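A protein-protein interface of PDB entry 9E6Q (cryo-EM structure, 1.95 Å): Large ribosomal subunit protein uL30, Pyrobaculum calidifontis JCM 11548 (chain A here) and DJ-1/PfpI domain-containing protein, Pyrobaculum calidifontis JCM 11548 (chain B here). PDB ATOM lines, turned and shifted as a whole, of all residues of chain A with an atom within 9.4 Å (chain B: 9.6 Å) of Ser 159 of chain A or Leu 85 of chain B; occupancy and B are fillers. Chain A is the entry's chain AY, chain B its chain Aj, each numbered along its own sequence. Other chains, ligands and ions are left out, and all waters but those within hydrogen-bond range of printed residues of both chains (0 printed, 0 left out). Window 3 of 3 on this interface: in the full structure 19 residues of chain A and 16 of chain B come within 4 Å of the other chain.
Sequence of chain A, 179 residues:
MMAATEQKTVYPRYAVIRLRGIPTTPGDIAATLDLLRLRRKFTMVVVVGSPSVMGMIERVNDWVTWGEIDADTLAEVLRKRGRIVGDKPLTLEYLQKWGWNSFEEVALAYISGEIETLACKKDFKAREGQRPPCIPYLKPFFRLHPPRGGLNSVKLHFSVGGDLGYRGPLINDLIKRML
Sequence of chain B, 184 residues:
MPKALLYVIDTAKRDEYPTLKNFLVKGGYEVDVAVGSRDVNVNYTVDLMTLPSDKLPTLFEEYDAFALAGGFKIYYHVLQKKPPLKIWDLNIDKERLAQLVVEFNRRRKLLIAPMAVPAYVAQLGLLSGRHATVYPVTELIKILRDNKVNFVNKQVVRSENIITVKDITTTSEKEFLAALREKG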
ATOM      1  N   ASN A  61     -15.552  12.708  -9.857  1.00  0.00           N
ATOM      2  CA  ASN A  61     -15.570  13.345  -8.544  1.00  0.00           C
ATOM      3  C   ASN A  61     -14.179  13.741  -8.066  1.00  0.00           C
ATOM      4  O   ASN A  61     -14.035  14.730  -7.345  1.00  0.00           O
ATOM      5  CB  ASN A  61     -16.218  12.418  -7.525  1.00  0.00           C
ATOM      6  CG  ASN A  61     -16.844  13.163  -6.379  1.00  0.00           C
ATOM      7  OD1 ASN A  61     -17.594  14.112  -6.575  1.00  0.00           O
ATOM      8  ND2 ASN A  61     -16.523  12.747  -5.167  1.00  0.00           N
ATOM      9  N   ASP A  62     -13.148  13.003  -8.453  1.00  0.00           N
ATOM     10  CA  ASP A  62     -11.800  13.277  -7.983  1.00  0.00           C
ATOM     11  C   ASP A  62     -11.068  14.298  -8.839  1.00  0.00           C
ATOM     12  O   ASP A  62      -9.896  14.572  -8.580  1.00  0.00           O
ATOM     13  CB  ASP A  62     -10.990  11.983  -7.912  1.00  0.00           C
ATOM     14  CG  ASP A  62     -11.777  10.842  -7.317  1.00  0.00           C
ATOM     15  OD1 ASP A  62     -12.098   9.888  -8.050  1.00  0.00           O
ATOM     16  OD2 ASP A  62     -12.075  10.897  -6.112  1.00  0.00           O
ATOM     17  N   THR A  65     -14.915  19.973  -8.562  1.00  0.00           N
ATOM     18  CA  THR A  65     -15.695  20.300  -7.381  1.00  0.00           C
ATOM     19  C   THR A  65     -17.017  20.880  -7.855  1.00  0.00           C
ATOM     20  O   THR A  65     -17.083  21.506  -8.911  1.00  0.00           O
ATOM     21  CB  THR A  65     -14.961  21.272  -6.446  1.00  0.00           C
ATOM     22  OG1 THR A  65     -15.659  21.354  -5.204  1.00  0.00           O
ATOM     23  CG2 THR A  65     -14.841  22.654  -7.051  1.00  0.00           C
ATOM     24  N   ASN A 152      -7.416  24.777  -0.785  1.00  0.00           N
ATOM     25  CA  ASN A 152      -6.819  24.015   0.304  1.00  0.00           C
ATOM     26  C   ASN A 152      -5.900  22.925  -0.228  1.00  0.00           C
ATOM     27  O   ASN A 152      -4.732  22.846   0.161  1.00  0.00           O
ATOM     28  CB  ASN A 152      -7.910  23.412   1.181  1.00  0.00           C
ATOM     29  CG  ASN A 152      -8.460  24.399   2.175  1.00  0.00           C
ATOM     30  OD1 ASN A 152      -7.847  25.423   2.451  1.00  0.00           O
ATOM     31  ND2 ASN A 152      -9.628  24.100   2.717  1.00  0.00           N
ATOM     32  N   SER A 153      -6.414  22.071  -1.106  1.00  0.00           N
ATOM     33  CA  SER A 153      -5.613  21.047  -1.760  1.00  0.00           C
ATOM     34  C   SER A 153      -6.394  20.451  -2.917  1.00  0.00           C
ATOM     35  O   SER A 153      -7.514  19.975  -2.725  1.00  0.00           O
ATOM     36  CB  SER A 153      -5.212  19.949  -0.776  1.00  0.00           C
ATOM     37  OG  SER A 153      -4.749  18.801  -1.458  1.00  0.00           O
ATOM     38  N   LEU A 156      -7.001  16.394  -2.299  1.00  0.00           N
ATOM     39  CA  LEU A 156      -7.816  15.833  -1.236  1.00  0.00           C
ATOM     40  C   LEU A 156      -9.271  16.216  -1.445  1.00  0.00           C
ATOM     41  O   LEU A 156      -9.578  17.251  -2.038  1.00  0.00           O
ATOM     42  CB  LEU A 156      -7.355  16.312   0.141  1.00  0.00           C
ATOM     43  CG  LEU A 156      -5.984  15.858   0.625  1.00  0.00           C
ATOM     44  CD1 LEU A 156      -5.690  16.457   1.984  1.00  0.00           C
ATOM     45  CD2 LEU A 156      -5.905  14.349   0.680  1.00  0.00           C
ATOM     46  N   HIS A 157     -10.164  15.362  -0.963  1.00  0.00           N
ATOM     47  CA  HIS A 157     -11.590  15.627  -1.063  1.00  0.00           C
ATOM     48  C   HIS A 157     -12.002  16.725  -0.095  1.00  0.00           C
ATOM     49  O   HIS A 157     -11.448  16.852   0.996  1.00  0.00           O
ATOM     50  CB  HIS A 157     -12.384  14.356  -0.773  1.00  0.00           C
ATOM     51  CG  HIS A 157     -12.473  13.424  -1.938  1.00  0.00           C
ATOM     52  ND1 HIS A 157     -13.521  12.548  -2.111  1.00  0.00           N
ATOM     53  CD2 HIS A 157     -11.641  13.227  -2.985  1.00  0.00           C
ATOM     54  CE1 HIS A 157     -13.331  11.853  -3.216  1.00  0.00           C
ATOM     55  NE2 HIS A 157     -12.196  12.244  -3.764  1.00  0.00           N
ATOM     56  N   PHE A 158     -13.001  17.510  -0.498  1.00  0.00           N
ATOM     57  CA  PHE A 158     -13.508  18.576   0.356  1.00  0.00           C
ATOM     58  C   PHE A 158     -13.985  18.049   1.699  1.00  0.00           C
ATOM     59  O   PHE A 158     -13.978  18.782   2.691  1.00  0.00           O
ATOM     60  CB  PHE A 158     -14.647  19.313  -0.352  1.00  0.00           C
ATOM     61  CG  PHE A 158     -15.257  20.413   0.459  1.00  0.00           C
ATOM     62  CD1 PHE A 158     -14.662  21.654   0.527  1.00  0.00           C
ATOM     63  CD2 PHE A 158     -16.433  20.205   1.151  1.00  0.00           C
ATOM     64  CE1 PHE A 158     -15.226  22.659   1.270  1.00  0.00           C
ATOM     65  CE2 PHE A 158     -16.995  21.207   1.896  1.00  0.00           C
ATOM     66  CZ  PHE A 158     -16.392  22.432   1.956  1.00  0.00           C
ATOM     67  N   SER A 159     -14.401  16.786   1.753  1.00  0.00           N
ATOM     68  CA  SER A 159     -14.953  16.220   2.977  1.00  0.00           C
ATOM     69  C   SER A 159     -13.898  15.979   4.048  1.00  0.00           C
ATOM     70  O   SER A 159     -14.254  15.810   5.216  1.00  0.00           O
ATOM     71  CB  SER A 159     -15.673  14.915   2.669  1.00  0.00           C
ATOM     72  OG  SER A 159     -14.860  14.066   1.891  1.00  0.00           O
ATOM     73  N   VAL A 160     -12.619  15.943   3.688  1.00  0.00           N
ATOM     74  CA  VAL A 160     -11.567  15.776   4.683  1.00  0.00           C
ATOM     75  C   VAL A 160     -10.606  16.953   4.627  1.00  0.00           C
ATOM     76  O   VAL A 160      -9.435  16.826   4.995  1.00  0.00           O
ATOM     77  CB  VAL A 160     -10.819  14.445   4.503  1.00  0.00           C
ATOM     78  CG1 VAL A 160     -11.710  13.286   4.893  1.00  0.00           C
ATOM     79  CG2 VAL A 160     -10.328  14.287   3.083  1.00  0.00           C
ATOM     80  N   GLY A 161     -11.088  18.105   4.178  1.00  0.00           N
ATOM     81  CA  GLY A 161     -10.317  19.326   4.219  1.00  0.00           C
ATOM     82  C   GLY A 161      -9.636  19.736   2.936  1.00  0.00           C
ATOM     83  O   GLY A 161      -8.852  20.689   2.956  1.00  0.00           O
ATOM     84  N   GLY A 162      -9.895  19.057   1.832  1.00  0.00           N
ATOM     85  CA  GLY A 162      -9.368  19.420   0.541  1.00  0.00           C
ATOM     86  C   GLY A 162     -10.339  20.267  -0.248  1.00  0.00           C
ATOM     87  O   GLY A 162     -11.099  21.066   0.305  1.00  0.00           O
ATOM     88  N   ASP A 163     -10.327  20.087  -1.562  1.00  0.00           N
ATOM     89  CA  ASP A 163     -11.183  20.871  -2.432  1.00  0.00           C
ATOM     90  C   ASP A 163     -11.987  20.064  -3.434  1.00  0.00           C
ATOM     91  O   ASP A 163     -12.858  20.639  -4.087  1.00  0.00           O
ATOM     92  CB  ASP A 163     -10.350  21.910  -3.194  1.00  0.00           C
ATOM     93  CG  ASP A 163      -9.743  22.945  -2.280  1.00  0.00           C
ATOM     94  OD1 ASP A 163     -10.461  23.878  -1.862  1.00  0.00           O
ATOM     95  OD2 ASP A 163      -8.543  22.822  -1.967  1.00  0.00           O
ATOM     96  N   LEU A 164     -11.734  18.770  -3.583  1.00  0.00           N
ATOM     97  CA  LEU A 164     -12.400  17.985  -4.607  1.00  0.00           C
ATOM     98  C   LEU A 164     -13.782  17.536  -4.149  1.00  0.00           C
ATOM     99  O   LEU A 164     -14.097  17.511  -2.962  1.00  0.00           O
ATOM    100  CB  LEU A 164     -11.560  16.765  -4.971  1.00  0.00           C
ATOM    101  CG  LEU A 164     -10.134  17.044  -5.433  1.00  0.00           C
ATOM    102  CD1 LEU A 164      -9.308  15.780  -5.389  1.00  0.00           C
ATOM    103  CD2 LEU A 164     -10.145  17.625  -6.823  1.00  0.00           C
ATOM    104  N   GLY A 165     -14.608  17.174  -5.117  1.00  0.00           N
ATOM    105  CA  GLY A 165     -15.875  16.545  -4.829  1.00  0.00           C
ATOM    106  C   GLY A 165     -16.982  17.527  -4.493  1.00  0.00           C
ATOM    107  O   GLY A 165     -16.905  18.725  -4.748  1.00  0.00           O
ATOM    108  N   TYR A 166     -18.031  16.979  -3.897  1.00  0.00           N
ATOM    109  CA  TYR A 166     -19.231  17.741  -3.595  1.00  0.00           C
ATOM    110  C   TYR A 166     -18.952  18.781  -2.519  1.00  0.00           C
ATOM    111  O   TYR A 166     -18.412  18.466  -1.460  1.00  0.00           O
ATOM    112  CB  TYR A 166     -20.340  16.796  -3.146  1.00  0.00           C
ATOM    113  CG  TYR A 166     -21.616  17.473  -2.738  1.00  0.00           C
ATOM    114  CD1 TYR A 166     -22.336  18.230  -3.638  1.00  0.00           C
ATOM    115  CD2 TYR A 166     -22.104  17.350  -1.449  1.00  0.00           C
ATOM    116  CE1 TYR A 166     -23.503  18.842  -3.275  1.00  0.00           C
ATOM    117  CE2 TYR A 166     -23.274  17.964  -1.073  1.00  0.00           C
ATOM    118  CZ  TYR A 166     -23.967  18.711  -1.992  1.00  0.00           C
ATOM    119  OH  TYR A 166     -25.132  19.328  -1.629  1.00  0.00           O
ATOM    120  N   ARG A 167     -19.335  20.020  -2.796  1.00  0.00           N
ATOM    121  CA  ARG A 167     -19.076  21.148  -1.922  1.00  0.00           C
ATOM    122  C   ARG A 167     -20.343  21.764  -1.351  1.00  0.00           C
ATOM    123  O   ARG A 167     -20.259  22.545  -0.403  1.00  0.00           O
ATOM    124  CB  ARG A 167     -18.287  22.217  -2.692  1.00  0.00           C
ATOM    125  CG  ARG A 167     -17.669  23.283  -1.855  1.00  0.00           C
ATOM    126  CD  ARG A 167     -16.840  24.202  -2.699  1.00  0.00           C
ATOM    127  NE  ARG A 167     -15.632  23.534  -3.153  1.00  0.00           N
ATOM    128  CZ  ARG A 167     -14.407  23.899  -2.811  1.00  0.00           C
ATOM    129  NH1 ARG A 167     -14.190  24.947  -2.040  1.00  0.00           N
ATOM    130  NH2 ARG A 167     -13.376  23.195  -3.258  1.00  0.00           N
ATOM    131  N   GLY A 168     -21.505  21.429  -1.893  1.00  0.00           N
ATOM    132  CA  GLY A 168     -22.743  22.020  -1.458  1.00  0.00           C
ATOM    133  C   GLY A 168     -22.851  23.462  -1.887  1.00  0.00           C
ATOM    134  O   GLY A 168     -22.309  23.865  -2.918  1.00  0.00           O
ATOM    135  N   PRO A 169     -23.549  24.278  -1.097  1.00  0.00           N
ATOM    136  CA  PRO A 169     -23.696  25.697  -1.450  1.00  0.00           C
ATOM    137  C   PRO A 169     -22.400  26.474  -1.401  1.00  0.00           C
ATOM    138  O   PRO A 169     -22.368  27.606  -1.886  1.00  0.00           O
ATOM    139  CB  PRO A 169     -24.691  26.225  -0.412  1.00  0.00           C
ATOM    140  CG  PRO A 169     -25.119  25.072   0.383  1.00  0.00           C
ATOM    141  CD  PRO A 169     -24.172  23.956   0.190  1.00  0.00           C
ATOM    142  N   LEU A 170     -21.337  25.912  -0.830  1.00  0.00           N
ATOM    143  CA  LEU A 170     -20.052  26.592  -0.791  1.00  0.00           C
ATOM    144  C   LEU A 170     -19.426  26.747  -2.168  1.00  0.00           C
ATOM    145  O   LEU A 170     -18.425  27.452  -2.290  1.00  0.00           O
ATOM    146  CB  LEU A 170     -19.098  25.845   0.132  1.00  0.00           C
ATOM    147  CG  LEU A 170     -19.131  26.254   1.601  1.00  0.00           C
ATOM    148  CD1 LEU A 170     -18.212  25.384   2.410  1.00  0.00           C
ATOM    149  CD2 LEU A 170     -18.740  27.707   1.750  1.00  0.00           C
ATOM    150  N   ASP B  10     -24.880  27.769  13.821  1.00  0.00           N
ATOM    151  CA  ASP B  10     -23.773  27.243  13.043  1.00  0.00           C
ATOM    152  C   ASP B  10     -22.827  28.381  12.694  1.00  0.00           C
ATOM    153  O   ASP B  10     -23.230  29.542  12.610  1.00  0.00           O
ATOM    154  CB  ASP B  10     -24.297  26.544  11.783  1.00  0.00           C
ATOM    155  CG  ASP B  10     -23.199  25.951  10.935  1.00  0.00           C
ATOM    156  OD1 ASP B  10     -22.579  24.957  11.359  1.00  0.00           O
ATOM    157  OD2 ASP B  10     -22.979  26.461   9.822  1.00  0.00           O
ATOM    158  N   ALA B  12     -20.307  27.546  10.081  1.00  0.00           N
ATOM    159  CA  ALA B  12     -19.607  27.083   8.886  1.00  0.00           C
ATOM    160  C   ALA B  12     -19.557  28.171   7.826  1.00  0.00           C
ATOM    161  O   ALA B  12     -18.546  28.326   7.134  1.00  0.00           O
ATOM    162  CB  ALA B  12     -20.265  25.822   8.334  1.00  0.00           C
ATOM    163  N   LYS B  13     -20.643  28.918   7.668  1.00  0.00           N
ATOM    164  CA  LYS B  13     -20.602  30.166   6.916  1.00  0.00           C
ATOM    165  C   LYS B  13     -19.792  31.158   7.736  1.00  0.00           C
ATOM    166  O   LYS B  13     -20.250  31.651   8.768  1.00  0.00           O
ATOM    167  CB  LYS B  13     -22.011  30.674   6.642  1.00  0.00           C
ATOM    168  CG  LYS B  13     -22.059  31.808   5.648  1.00  0.00           C
ATOM    169  CD  LYS B  13     -22.055  31.277   4.234  1.00  0.00           C
ATOM    170  CE  LYS B  13     -22.871  32.159   3.316  1.00  0.00           C
ATOM    171  NZ  LYS B  13     -22.067  32.644   2.163  1.00  0.00           N
ATOM    172  N   PHE B  72     -25.052  26.209   7.145  1.00  0.00           N
ATOM    173  CA  PHE B  72     -25.364  25.027   6.360  1.00  0.00           C
ATOM    174  C   PHE B  72     -26.065  23.948   7.167  1.00  0.00           C
ATOM    175  O   PHE B  72     -26.555  22.984   6.576  1.00  0.00           O
ATOM    176  CB  PHE B  72     -24.080  24.483   5.745  1.00  0.00           C
ATOM    177  CG  PHE B  72     -23.307  25.514   4.989  1.00  0.00           C
ATOM    178  CD1 PHE B  72     -23.962  26.465   4.233  1.00  0.00           C
ATOM    179  CD2 PHE B  72     -21.935  25.572   5.079  1.00  0.00           C
ATOM    180  CE1 PHE B  72     -23.259  27.426   3.552  1.00  0.00           C
ATOM    181  CE2 PHE B  72     -21.229  26.537   4.396  1.00  0.00           C
ATOM    182  CZ  PHE B  72     -21.893  27.462   3.635  1.00  0.00           C
ATOM    183  N   LYS B  73     -26.121  24.085   8.491  1.00  0.00           N
ATOM    184  CA  LYS B  73     -26.884  23.142   9.300  1.00  0.00           C
ATOM    185  C   LYS B  73     -28.367  23.218   8.970  1.00  0.00           C
ATOM    186  O   LYS B  73     -29.029  22.194   8.789  1.00  0.00           O
ATOM    187  CB  LYS B  73     -26.654  23.415  10.785  1.00  0.00           C
ATOM    188  CG  LYS B  73     -25.311  22.974  11.313  1.00  0.00           C
ATOM    189  CD  LYS B  73     -25.225  23.191  12.810  1.00  0.00           C
ATOM    190  CE  LYS B  73     -23.860  22.827  13.349  1.00  0.00           C
ATOM    191  NZ  LYS B  73     -23.761  23.092  14.804  1.00  0.00           N
ATOM    192  N   TYR B  76     -29.212  21.892   5.190  1.00  0.00           N
ATOM    193  CA  TYR B  76     -29.345  20.465   4.933  1.00  0.00           C
ATOM    194  C   TYR B  76     -30.447  19.819   5.752  1.00  0.00           C
ATOM    195  O   TYR B  76     -30.883  18.716   5.413  1.00  0.00           O
ATOM    196  CB  TYR B  76     -28.010  19.762   5.169  1.00  0.00           C
ATOM    197  CG  TYR B  76     -27.079  19.949   4.000  1.00  0.00           C
ATOM    198  CD1 TYR B  76     -27.245  19.211   2.840  1.00  0.00           C
ATOM    199  CD2 TYR B  76     -26.067  20.887   4.039  1.00  0.00           C
ATOM    200  CE1 TYR B  76     -26.418  19.389   1.764  1.00  0.00           C
ATOM    201  CE2 TYR B  76     -25.232  21.072   2.966  1.00  0.00           C
ATOM    202  CZ  TYR B  76     -25.413  20.320   1.830  1.00  0.00           C
ATOM    203  OH  TYR B  76     -24.583  20.497   0.759  1.00  0.00           O
ATOM    204  N   LYS B  81     -31.281  16.249   3.440  1.00  0.00           N
ATOM    205  CA  LYS B  81     -30.189  15.719   2.644  1.00  0.00           C
ATOM    206  C   LYS B  81     -28.963  15.538   3.527  1.00  0.00           C
ATOM    207  O   LYS B  81     -28.806  16.220   4.542  1.00  0.00           O
ATOM    208  CB  LYS B  81     -29.872  16.657   1.479  1.00  0.00           C
ATOM    209  CG  LYS B  81     -29.120  16.029   0.332  1.00  0.00           C
ATOM    210  CD  LYS B  81     -28.673  17.091  -0.663  1.00  0.00           C
ATOM    211  CE  LYS B  81     -27.476  16.629  -1.483  1.00  0.00           C
ATOM    212  NZ  LYS B  81     -26.519  15.811  -0.692  1.00  0.00           N
ATOM    213  N   LYS B  82     -28.104  14.604   3.147  1.00  0.00           N
ATOM    214  CA  LYS B  82     -26.895  14.349   3.917  1.00  0.00           C
ATOM    215  C   LYS B  82     -25.823  15.369   3.557  1.00  0.00           C
ATOM    216  O   LYS B  82     -25.464  15.485   2.383  1.00  0.00           O
ATOM    217  CB  LYS B  82     -26.382  12.942   3.662  1.00  0.00           C
ATOM    218  CG  LYS B  82     -25.471  12.421   4.750  1.00  0.00           C
ATOM    219  CD  LYS B  82     -25.165  10.950   4.565  1.00  0.00           C
ATOM    220  CE  LYS B  82     -23.674  10.693   4.642  1.00  0.00           C
ATOM    221  NZ  LYS B  82     -22.928  11.515   3.651  1.00  0.00           N
ATOM    222  N   PRO B  83     -25.290  16.113   4.517  1.00  0.00           N
ATOM    223  CA  PRO B  83     -24.273  17.108   4.207  1.00  0.00           C
ATOM    224  C   PRO B  83     -22.946  16.449   3.883  1.00  0.00           C
ATOM    225  O   PRO B  83     -22.716  15.289   4.246  1.00  0.00           O
ATOM    226  CB  PRO B  83     -24.184  17.944   5.492  1.00  0.00           C
ATOM    227  CG  PRO B  83     -24.902  17.181   6.540  1.00  0.00           C
ATOM    228  CD  PRO B  83     -25.505  15.954   5.962  1.00  0.00           C
ATOM    229  N   PRO B  84     -22.052  17.150   3.182  1.00  0.00           N
ATOM    230  CA  PRO B  84     -20.724  16.582   2.908  1.00  0.00           C
ATOM    231  C   PRO B  84     -19.817  16.521   4.121  1.00  0.00           C
ATOM    232  O   PRO B  84     -18.808  15.809   4.075  1.00  0.00           O
ATOM    233  CB  PRO B  84     -20.148  17.512   1.835  1.00  0.00           C
ATOM    234  CG  PRO B  84     -21.066  18.663   1.723  1.00  0.00           C
ATOM    235  CD  PRO B  84     -22.222  18.501   2.628  1.00  0.00           C
ATOM    236  N   LEU B  85     -20.130  17.237   5.194  1.00  0.00           N
ATOM    237  CA  LEU B  85     -19.356  17.208   6.424  1.00  0.00           C
ATOM    238  C   LEU B  85     -20.266  16.795   7.567  1.00  0.00           C
ATOM    239  O   LEU B  85     -21.435  17.178   7.603  1.00  0.00           O
ATOM    240  CB  LEU B  85     -18.739  18.572   6.726  1.00  0.00           C
ATOM    241  CG  LEU B  85     -17.751  19.150   5.721  1.00  0.00           C
ATOM    242  CD1 LEU B  85     -17.268  20.500   6.192  1.00  0.00           C
ATOM    243  CD2 LEU B  85     -16.588  18.210   5.539  1.00  0.00           C
ATOM    244  N   LYS B  86     -19.732  16.004   8.497  1.00  0.00           N
ATOM    245  CA  LYS B  86     -20.519  15.615   9.662  1.00  0.00           C
ATOM    246  C   LYS B  86     -20.801  16.803  10.571  1.00  0.00           C
ATOM    247  O   LYS B  86     -21.833  16.833  11.245  1.00  0.00           O
ATOM    248  CB  LYS B  86     -19.806  14.512  10.435  1.00  0.00           C
ATOM    249  CG  LYS B  86     -20.105  13.125   9.920  1.00  0.00           C
ATOM    250  CD  LYS B  86     -19.025  12.142  10.325  1.00  0.00           C
ATOM    251  CE  LYS B  86     -19.339  10.747   9.810  1.00  0.00           C
ATOM    252  NZ  LYS B  86     -19.874   9.868  10.887  1.00  0.00           N
ATOM    253  N   ILE B  87     -19.911  17.796  10.591  1.00  0.00           N
ATOM    254  CA  ILE B  87     -20.122  18.972  11.423  1.00  0.00           C
ATOM    255  C   ILE B  87     -21.274  19.830  10.929  1.00  0.00           C
ATOM    256  O   ILE B  87     -21.728  20.721  11.651  1.00  0.00           O
ATOM    257  CB  ILE B  87     -18.846  19.827  11.506  1.00  0.00           C
ATOM    258  CG1 ILE B  87     -18.098  19.791  10.181  1.00  0.00           C
ATOM    259  CG2 ILE B  87     -17.956  19.341  12.627  1.00  0.00           C
ATOM    260  CD1 ILE B  87     -17.087  20.887  10.032  1.00  0.00           C
ATOM    261  N   TRP B  88     -21.751  19.608   9.708  1.00  0.00           N
ATOM    262  CA  TRP B  88     -22.900  20.339   9.200  1.00  0.00           C
ATOM    263  C   TRP B  88     -24.223  19.699   9.592  1.00  0.00           C
ATOM    264  O   TRP B  88     -25.274  20.185   9.171  1.00  0.00           O
ATOM    265  CB  TRP B  88     -22.822  20.464   7.681  1.00  0.00           C
ATOM    266  CG  TRP B  88     -21.709  21.326   7.202  1.00  0.00           C
ATOM    267  CD1 TRP B  88     -20.765  21.936   7.961  1.00  0.00           C
ATOM    268  CD2 TRP B  88     -21.417  21.667   5.845  1.00  0.00           C
ATOM    269  NE1 TRP B  88     -19.900  22.639   7.166  1.00  0.00           N
ATOM    270  CE2 TRP B  88     -20.281  22.490   5.859  1.00  0.00           C
ATOM    271  CE3 TRP B  88     -22.005  21.353   4.621  1.00  0.00           C
ATOM    272  CZ2 TRP B  88     -19.722  23.004   4.699  1.00  0.00           C
ATOM    273  CZ3 TRP B  88     -21.451  21.867   3.474  1.00  0.00           C
ATOM    274  CH2 TRP B  88     -20.322  22.681   3.519  1.00  0.00           C
ATOM    275  N   ASP B  89     -24.195  18.612  10.352  1.00  0.00           N
ATOM    276  CA  ASP B  89     -25.413  18.046  10.910  1.00  0.00           C
ATOM    277  C   ASP B  89     -26.025  18.997  11.927  1.00  0.00           C
ATOM    278  O   ASP B  89     -25.322  19.688  12.665  1.00  0.00           O
ATOM    279  CB  ASP B  89     -25.126  16.708  11.584  1.00  0.00           C
ATOM    280  CG  ASP B  89     -24.824  15.612  10.598  1.00  0.00           C
ATOM    281  OD1 ASP B  89     -25.361  15.663   9.474  1.00  0.00           O
ATOM    282  OD2 ASP B  89     -24.059  14.690  10.945  1.00  0.00           O
ATOM    283  N   LEU B  90     -27.353  19.018  11.969  1.00  0.00           N
ATOM    284  CA  LEU B  90     -28.082  19.837  12.934  1.00  0.00           C
ATOM    285  C   LEU B  90     -28.034  19.134  14.283  1.00  0.00           C
ATOM    286  O   LEU B  90     -28.824  18.231  14.555  1.00  0.00           O
ATOM    287  CB  LEU B  90     -29.513  20.068  12.468  1.00  0.00           C
ATOM    288  CG  LEU B  90     -30.292  21.199  13.135  1.00  0.00           C
ATOM    289  CD1 LEU B  90     -29.494  22.482  13.151  1.00  0.00           C
ATOM    290  CD2 LEU B  90     -31.606  21.411  12.431  1.00  0.00           C
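OD2 of Asp 10 of chain B sits at hydrogen-bond distance from N of Phe 72 of chain B (3.4 Å).
The backbone NH (N) of Lys 81 of chain B sits at hydrogen-bond distance from the backbone carbonyl oxygen (O) of Tyr 76 of chain B, at 3.2 Å.
The backbone NH (N) of Phe 158 of chain A lies within hydrogen-bond range of the backbone carbonyl oxygen (O) of Leu 164 of chain A, 2.7 Å away.
OD1 of Asp 163 of chain A lies within salt-bridge range of NH2 of Arg 167 of chain A (3.3 Å).
The side-chain hydroxyl of Thr 65 of chain A is in hydrogen-bond range of the guanidinium group of Arg 167 of chain A.
Printed residues of chain A that touch a printed residue of chain B: Phe 158, Ser 159, Tyr 166, Arg 167, Gly 168, Pro 169 and Leu 170.
Hydrophobic or aromatic side chains of chain A within 4 Å of the printed part of chain B: Phe 158, Tyr 166, Pro 169 and Leu 170.
Printed residues of chain B that touch a printed residue of chain A: Phe 72, Tyr 76, Lys 81, Pro 84, Leu 85 and Trp 88.
Hydrophobic or aromatic side chains of chain B that line the printed part of chain A: Phe 72, Tyr 76, Pro 84, Leu 85 and Trp 88.
Along chain B the printed residues that touch a printed residue of chain A span positions 72 to 88.
The side-chain hydroxyl (OH) of Tyr 76 of chain B lies within hydrogen-bond range of the side-chain hydroxyl (OH) of Tyr 166 of chain A.
Ser 159 of chain A touches two residues of chain B.
Pro 83 of chain B touches none of the printed residues of chain A.
Pro 84 of chain B touches just these residues of chain A: Ser 159 (3.6 Å) and Tyr 166 (3.6 Å).
Of the printed residues of chain B, Leu 170 of chain A touches Phe 72 and Trp 88.
Printed residues of chain B within 4 Å of Arg 167 of chain A: Trp 88.
Of the printed residues of chain B, Tyr 166 of chain A touches Tyr 76, Lys 81 and Pro 84.
Thr 65 of chain A touches none of the printed residues of chain B.
Lys 82 of chain B touches none of the printed residues of chain A.
Among the printed residues, pairs that only touch across the chains: Phe 158 of chain A with Leu 85 of chain B, Phe 158 of chain A with Trp 88 of chain B, Ser 159 of chain A with Pro 84 of chain B, Ser 159 of chain A with Leu 85 of chain B, Tyr 166 of chain A with Lys 81 of chain B, Tyr 166 of chain A with Pro 84 of chain B, Arg 167 of chain A with Trp 88 of chain B, Gly 168 of chain A with Tyr 76 of chain B, Pro 169 of chain A with Tyr 76 of chain B, Leu 170 of chain A with Phe 72 of chain B and Leu 170 of chain A with Trp 88 of chain B.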
